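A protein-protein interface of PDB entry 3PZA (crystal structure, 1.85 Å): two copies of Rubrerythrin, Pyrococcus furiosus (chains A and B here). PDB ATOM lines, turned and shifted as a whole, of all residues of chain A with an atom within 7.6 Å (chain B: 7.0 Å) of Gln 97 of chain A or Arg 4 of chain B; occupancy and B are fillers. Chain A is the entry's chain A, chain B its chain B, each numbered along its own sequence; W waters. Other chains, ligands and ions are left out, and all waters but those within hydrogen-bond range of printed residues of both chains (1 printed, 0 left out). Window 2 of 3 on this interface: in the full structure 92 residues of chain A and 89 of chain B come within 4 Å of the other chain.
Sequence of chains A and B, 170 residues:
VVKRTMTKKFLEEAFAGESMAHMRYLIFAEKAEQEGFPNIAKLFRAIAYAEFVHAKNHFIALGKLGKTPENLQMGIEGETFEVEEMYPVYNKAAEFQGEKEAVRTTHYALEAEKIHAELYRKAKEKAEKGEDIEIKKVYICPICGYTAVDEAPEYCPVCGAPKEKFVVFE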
ATOM      1  N   ASN A  91      11.011  -5.897 -33.169  1.00  0.00           N
ATOM      2  CA  ASN A  91      11.051  -4.427 -33.386  1.00  0.00           C
ATOM      3  C   ASN A  91       9.596  -3.931 -33.453  1.00  0.00           C
ATOM      4  O   ASN A  91       9.265  -2.898 -32.896  1.00  0.00           O
ATOM      5  CB  ASN A  91      11.756  -4.145 -34.706  1.00  0.00           C
ATOM      6  CG  ASN A  91      11.753  -2.676 -35.085  1.00  0.00           C
ATOM      7  OD1 ASN A  91      10.884  -2.276 -35.870  1.00  0.00           O
ATOM      8  ND2 ASN A  91      12.704  -1.857 -34.539  1.00  0.00           N
ATOM      9  N   LYS A  92       8.700  -4.646 -34.151  1.00  0.00           N
ATOM     10  CA  LYS A  92       7.321  -4.134 -34.303  1.00  0.00           C
ATOM     11  C   LYS A  92       6.621  -4.202 -32.966  1.00  0.00           C
ATOM     12  O   LYS A  92       5.791  -3.320 -32.596  1.00  0.00           O
ATOM     13  CB  LYS A  92       6.570  -5.074 -35.260  1.00  0.00           C
ATOM     14  CG  LYS A  92       5.110  -4.782 -35.520  1.00  0.00           C
ATOM     15  CD  LYS A  92       4.798  -3.377 -36.007  1.00  0.00           C
ATOM     16  CE  LYS A  92       5.503  -2.998 -37.220  1.00  0.00           C
ATOM     17  NZ  LYS A  92       4.755  -1.679 -37.598  1.00  0.00           N
ATOM     18  N   ALA A  93       6.935  -5.233 -32.186  1.00  0.00           N
ATOM     19  CA  ALA A  93       6.348  -5.328 -30.852  1.00  0.00           C
ATOM     20  C   ALA A  93       6.810  -4.186 -29.934  1.00  0.00           C
ATOM     21  O   ALA A  93       6.001  -3.636 -29.149  1.00  0.00           O
ATOM     22  CB  ALA A  93       6.693  -6.670 -30.178  1.00  0.00           C
ATOM     23  N   ALA A  94       8.100  -3.860 -29.986  1.00  0.00           N
ATOM     24  CA  ALA A  94       8.634  -2.752 -29.182  1.00  0.00           C
ATOM     25  C   ALA A  94       7.963  -1.462 -29.614  1.00  0.00           C
ATOM     26  O   ALA A  94       7.587  -0.584 -28.756  1.00  0.00           O
ATOM     27  CB  ALA A  94      10.166  -2.652 -29.359  1.00  0.00           C
ATOM     28  N   GLU A  95       7.730  -1.336 -30.919  1.00  0.00           N
ATOM     29  CA  GLU A  95       7.064  -0.127 -31.359  1.00  0.00           C
ATOM     30  C   GLU A  95       5.629  -0.084 -30.876  1.00  0.00           C
ATOM     31  O   GLU A  95       5.162   0.967 -30.417  1.00  0.00           O
ATOM     32  CB  GLU A  95       7.152  -0.002 -32.907  1.00  0.00           C
ATOM     33  CG  GLU A  95       6.138   0.996 -33.468  1.00  0.00           C
ATOM     34  CD  GLU A  95       6.013   0.809 -34.990  1.00  0.00           C
ATOM     35  OE1 GLU A  95       6.912   1.312 -35.712  1.00  0.00           O
ATOM     36  OE2 GLU A  95       5.054   0.144 -35.448  1.00  0.00           O
ATOM     37  N   PHE A  96       4.909  -1.220 -30.982  1.00  0.00           N
ATOM     38  CA  PHE A  96       3.542  -1.332 -30.507  1.00  0.00           C
ATOM     39  C   PHE A  96       3.455  -1.030 -29.005  1.00  0.00           C
ATOM     40  O   PHE A  96       2.470  -0.471 -28.534  1.00  0.00           O
ATOM     41  CB  PHE A  96       3.046  -2.764 -30.787  1.00  0.00           C
ATOM     42  CG  PHE A  96       1.661  -3.065 -30.316  1.00  0.00           C
ATOM     43  CD1 PHE A  96       1.446  -3.945 -29.251  1.00  0.00           C
ATOM     44  CD2 PHE A  96       0.563  -2.549 -31.012  1.00  0.00           C
ATOM     45  CE1 PHE A  96       0.210  -4.268 -28.890  1.00  0.00           C
ATOM     46  CE2 PHE A  96      -0.759  -2.850 -30.607  1.00  0.00           C
ATOM     47  CZ  PHE A  96      -0.941  -3.711 -29.551  1.00  0.00           C
ATOM     48  N   GLN A  97       4.442  -1.401 -28.218  1.00  0.00           N
ATOM     49  CA  GLN A  97       4.313  -1.180 -26.791  1.00  0.00           C
ATOM     50  C   GLN A  97       4.928   0.156 -26.398  1.00  0.00           C
ATOM     51  O   GLN A  97       5.075   0.387 -25.197  1.00  0.00           O
ATOM     52  CB  GLN A  97       5.058  -2.267 -25.966  1.00  0.00           C
ATOM     53  CG  GLN A  97       4.455  -3.672 -26.197  1.00  0.00           C
ATOM     54  CD  GLN A  97       4.695  -4.598 -25.050  1.00  0.00           C
ATOM     55  OE1 GLN A  97       5.851  -4.912 -24.708  1.00  0.00           O
ATOM     56  NE2 GLN A  97       3.584  -5.078 -24.430  1.00  0.00           N
ATOM     57  N   GLY A  98       5.358   0.933 -27.377  1.00  0.00           N
ATOM     58  CA  GLY A  98       5.949   2.298 -27.100  1.00  0.00           C
ATOM     59  C   GLY A  98       7.366   2.291 -26.476  1.00  0.00           C
ATOM     60  O   GLY A  98       7.753   3.308 -25.841  1.00  0.00           O
ATOM     61  N   GLU A  99       8.157   1.209 -26.612  1.00  0.00           N
ATOM     62  CA  GLU A  99       9.462   1.065 -25.880  1.00  0.00           C
ATOM     63  C   GLU A  99      10.559   1.529 -26.853  1.00  0.00           C
ATOM     64  O   GLU A  99      11.144   0.747 -27.668  1.00  0.00           O
ATOM     65  CB  GLU A  99       9.688  -0.413 -25.422  1.00  0.00           C
ATOM     66  CG  GLU A  99       8.747  -0.795 -24.241  1.00  0.00           C
ATOM     67  CD  GLU A  99       9.283  -0.263 -22.863  1.00  0.00           C
ATOM     68  OE1 GLU A  99       8.739  -0.631 -21.822  1.00  0.00           O
ATOM     69  OE2 GLU A  99      10.312   0.486 -22.786  1.00  0.00           O
ATOM     70  N   LYS A 100      10.766   2.846 -26.884  1.00  0.00           N
ATOM     71  CA  LYS A 100      11.661   3.393 -27.906  1.00  0.00           C
ATOM     72  C   LYS A 100      13.095   2.874 -27.827  1.00  0.00           C
ATOM     73  O   LYS A 100      13.779   2.787 -28.859  1.00  0.00           O
ATOM     74  CB  LYS A 100      11.711   4.953 -27.716  1.00  0.00           C
ATOM     75  CG  LYS A 100      10.291   5.624 -27.812  1.00  0.00           C
ATOM     76  CD  LYS A 100       9.316   5.029 -28.862  1.00  0.00           C
ATOM     77  CE  LYS A 100       7.951   5.827 -28.820  1.00  0.00           C
ATOM     78  NZ  LYS A 100       8.240   7.328 -28.991  1.00  0.00           N
ATOM     79  N   VAL A 103      13.072  -0.317 -29.534  1.00  0.00           N
ATOM     80  CA  VAL A 103      12.918  -0.118 -30.972  1.00  0.00           C
ATOM     81  C   VAL A 103      14.321   0.160 -31.578  1.00  0.00           C
ATOM     82  O   VAL A 103      14.651  -0.356 -32.636  1.00  0.00           O
ATOM     83  CB  VAL A 103      11.958   1.066 -31.267  1.00  0.00           C
ATOM     84  CG1 VAL A 103      12.109   1.489 -32.812  1.00  0.00           C
ATOM     85  CG2 VAL A 103      10.495   0.627 -31.038  1.00  0.00           C
ATOM     86  N   VAL B   1      15.141   2.634 -19.285  1.00  0.00           N
ATOM     87  CA  VAL B   1      15.122   1.145 -19.053  1.00  0.00           C
ATOM     88  C   VAL B   1      13.747   0.590 -19.551  1.00  0.00           C
ATOM     89  O   VAL B   1      12.720   1.204 -19.300  1.00  0.00           O
ATOM     90  CB  VAL B   1      15.246   0.771 -17.531  1.00  0.00           C
ATOM     91  CG1 VAL B   1      15.247  -0.732 -17.401  1.00  0.00           C
ATOM     92  CG2 VAL B   1      16.549   1.311 -16.916  1.00  0.00           C
ATOM     93  N   VAL B   2      13.747  -0.539 -20.265  1.00  0.00           N
ATOM     94  CA  VAL B   2      12.516  -1.141 -20.772  1.00  0.00           C
ATOM     95  C   VAL B   2      11.720  -1.703 -19.630  1.00  0.00           C
ATOM     96  O   VAL B   2      12.296  -2.448 -18.821  1.00  0.00           O
ATOM     97  CB  VAL B   2      12.873  -2.199 -21.795  1.00  0.00           C
ATOM     98  CG1 VAL B   2      11.590  -3.071 -22.174  1.00  0.00           C
ATOM     99  CG2 VAL B   2      13.528  -1.486 -23.062  1.00  0.00           C
ATOM    100  N   LYS B   3      10.397  -1.426 -19.576  1.00  0.00           N
ATOM    101  CA  LYS B   3       9.527  -1.886 -18.468  1.00  0.00           C
ATOM    102  C   LYS B   3       8.377  -2.860 -18.891  1.00  0.00           C
ATOM    103  O   LYS B   3       7.935  -3.700 -18.120  1.00  0.00           O
ATOM    104  CB  LYS B   3       8.944  -0.656 -17.784  1.00  0.00           C
ATOM    105  CG  LYS B   3      10.066   0.324 -17.256  1.00  0.00           C
ATOM    106  CD  LYS B   3       9.538   1.790 -17.027  1.00  0.00           C
ATOM    107  CE  LYS B   3       8.735   2.518 -18.269  1.00  0.00           C
ATOM    108  NZ  LYS B   3       7.319   2.982 -17.806  1.00  0.00           N
ATOM    109  N   ARG B   4       7.909  -2.758 -20.127  1.00  0.00           N
ATOM    110  CA  ARG B   4       6.737  -3.562 -20.516  1.00  0.00           C
ATOM    111  C   ARG B   4       7.173  -5.040 -20.593  1.00  0.00           C
ATOM    112  O   ARG B   4       8.282  -5.407 -21.056  1.00  0.00           O
ATOM    113  CB  ARG B   4       6.197  -3.090 -21.851  1.00  0.00           C
ATOM    114  CG  ARG B   4       5.557  -1.638 -21.922  1.00  0.00           C
ATOM    115  CD  ARG B   4       4.258  -1.531 -21.130  1.00  0.00           C
ATOM    116  NE  ARG B   4       3.250  -2.019 -22.000  1.00  0.00           N
ATOM    117  CZ  ARG B   4       2.610  -1.290 -22.921  1.00  0.00           C
ATOM    118  NH1 ARG B   4       1.730  -1.899 -23.663  1.00  0.00           N
ATOM    119  NH2 ARG B   4       2.786   0.043 -23.056  1.00  0.00           N
ATOM    120  N   THR B   5       6.313  -5.914 -20.093  1.00  0.00           N
ATOM    121  CA  THR B   5       6.656  -7.305 -19.937  1.00  0.00           C
ATOM    122  C   THR B   5       7.077  -8.005 -21.222  1.00  0.00           C
ATOM    123  O   THR B   5       8.081  -8.730 -21.194  1.00  0.00           O
ATOM    124  CB  THR B   5       5.503  -8.112 -19.261  1.00  0.00           C
ATOM    125  OG1 THR B   5       5.275  -7.464 -18.030  1.00  0.00           O
ATOM    126  CG2 THR B   5       5.985  -9.526 -18.840  1.00  0.00           C
ATOM    127  N   MET B   6       6.272  -7.873 -22.270  1.00  0.00           N
ATOM    128  CA  MET B   6       6.608  -8.630 -23.506  1.00  0.00           C
ATOM    129  C   MET B   6       7.907  -8.102 -24.097  1.00  0.00           C
ATOM    130  O   MET B   6       8.765  -8.897 -24.510  1.00  0.00           O
ATOM    131  CB  MET B   6       5.430  -8.502 -24.475  1.00  0.00           C
ATOM    132  CG  MET B   6       4.104  -9.128 -23.972  1.00  0.00           C
ATOM    133  SD  MET B   6       4.351 -10.915 -23.493  1.00  0.00           S
ATOM    134  CE  MET B   6       4.810 -11.698 -25.098  1.00  0.00           C
ATOM    135  N   THR B   7       8.093  -6.765 -24.197  1.00  0.00           N
ATOM    136  CA  THR B   7       9.334  -6.260 -24.782  1.00  0.00           C
ATOM    137  C   THR B   7      10.560  -6.638 -23.940  1.00  0.00           C
ATOM    138  O   THR B   7      11.635  -6.976 -24.452  1.00  0.00           O
ATOM    139  CB  THR B   7       9.238  -4.734 -25.019  1.00  0.00           C
ATOM    140  OG1 THR B   7       8.206  -4.475 -26.010  1.00  0.00           O
ATOM    141  CG2 THR B   7      10.591  -4.172 -25.544  1.00  0.00           C
ATOM    142  N   LYS B   8      10.429  -6.659 -22.622  1.00  0.00           N
ATOM    143  CA  LYS B   8      11.480  -7.133 -21.807  1.00  0.00           C
ATOM    144  C   LYS B   8      11.859  -8.595 -22.051  1.00  0.00           C
ATOM    145  O   LYS B   8      13.021  -8.968 -22.146  1.00  0.00           O
ATOM    146  CB  LYS B   8      11.050  -6.880 -20.316  1.00  0.00           C
ATOM    147  CG  LYS B   8      12.014  -7.336 -19.293  1.00  0.00           C
ATOM    148  CD  LYS B   8      11.561  -6.735 -17.907  1.00  0.00           C
ATOM    149  CE  LYS B   8      12.388  -7.497 -16.907  1.00  0.00           C
ATOM    150  NZ  LYS B   8      11.880  -7.282 -15.518  1.00  0.00           N
ATOM    151  N   LYS B   9      10.860  -9.471 -22.129  1.00  0.00           N
ATOM    152  CA  LYS B   9      11.108 -10.853 -22.431  1.00  0.00           C
ATOM    153  C   LYS B   9      11.796 -10.956 -23.821  1.00  0.00           C
ATOM    154  O   LYS B   9      12.730 -11.759 -23.947  1.00  0.00           O
ATOM    155  CB  LYS B   9       9.759 -11.591 -22.582  1.00  0.00           C
ATOM    156  CG  LYS B   9      10.011 -13.132 -22.848  1.00  0.00           C
ATOM    157  CD  LYS B   9       8.822 -13.991 -23.226  1.00  0.00           C
ATOM    158  CE  LYS B   9       9.293 -15.497 -23.134  1.00  0.00           C
ATOM    159  NZ  LYS B   9       8.169 -16.378 -23.440  1.00  0.00           N
ATOM    160  N   PHE B  10      11.312 -10.234 -24.825  1.00  0.00           N
ATOM    161  CA  PHE B  10      11.914 -10.302 -26.174  1.00  0.00           C
ATOM    162  C   PHE B  10      13.369  -9.849 -26.125  1.00  0.00           C
ATOM    163  O   PHE B  10      14.215 -10.459 -26.745  1.00  0.00           O
ATOM    164  CB  PHE B  10      11.113  -9.453 -27.182  1.00  0.00           C
ATOM    165  CG  PHE B  10       9.773 -10.019 -27.465  1.00  0.00           C
ATOM    166  CD1 PHE B  10       8.790  -9.216 -28.087  1.00  0.00           C
ATOM    167  CD2 PHE B  10       9.431 -11.359 -27.066  1.00  0.00           C
ATOM    168  CE1 PHE B  10       7.549  -9.737 -28.411  1.00  0.00           C
ATOM    169  CE2 PHE B  10       8.090 -11.881 -27.336  1.00  0.00           C
ATOM    170  CZ  PHE B  10       7.174 -11.058 -28.000  1.00  0.00           C
HETATM  171  O   HOH W   1       0.914  -4.730 -25.183  1.00  0.00           O
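The backbone carbonyl oxygen (O) of Gln 97 of chain A lies within hydrogen-bond range of the guanidinium group (NH2) of Arg 4 of chain B, at 3.2 Å. The side-chain hydroxyl (OG1) of Thr 7 of chain B lies within hydrogen-bond range of the side-chain amide oxygen (OE1) of Gln 97 of chain A (2.7 Å). The side-chain carboxylate (OE1) of Glu 99 of chain A lies within hydrogen-bond range of the backbone NH (N) of Lys 3 of chain B. OE1 of Glu 99 of chain A lies within hydrogen-bond range of N of Arg 4 of chain B (2.8 Å).
N of Glu 99 of chain A is in hydrogen-bond range of O of Ala 94 of chain A (2.9 Å).
Among the printed residues, merely in contact across the chains: Ala 93 of chain A with Thr 7 of chain B (3.9 Å), Ala 93 of chain A with Phe 10 of chain B (3.6 Å), Ala 94 of chain A with Thr 7 of chain B (3.6 Å), Gln 97 of chain A with Met 6 of chain B (3.6 Å), Glu 99 of chain A with Val 2 of chain B (3.4 Å) and Glu 99 of chain A with Thr 7 of chain B (3.9 Å).
Of the printed residues of chain B, Ala 94 of chain A touches Thr 7. Gln 97 of chain A touches just these residues of chain B: Arg 4 (3.2 Å), Met 6 (3.6 Å) and Thr 7 (2.7 Å). Of the printed residues of chain A, Arg 4 of chain B touches Gln 97 (3.2 Å) and Glu 99 (2.8 Å). Printed residues of chain A within 4 Å of Thr 7 of chain B: Ala 93, Ala 94, Gln 97 and Glu 99. Lys 9 of chain B touches none of the printed residues of chain A.
Of the 10 printed residues of chain B, 6 touch a printed residue of chain A. Hydrophobic or aromatic side chains of chain B that line the printed part of chain A: Val 2, Met 6 and Phe 10. Among the printed residues, 10 pairs touch across the chains.
No position is printed for both chains. Of the 10 pairs that touch across the chains among the printed residues, none has its exchanged pair printed and touching as well.
Water W1 bridges the side-chain amide nitrogen (NE2) of Gln 97 of chain A (2.8 Å) and the guanidinium group (NH1) of Arg 4 of chain B (3.3 Å).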
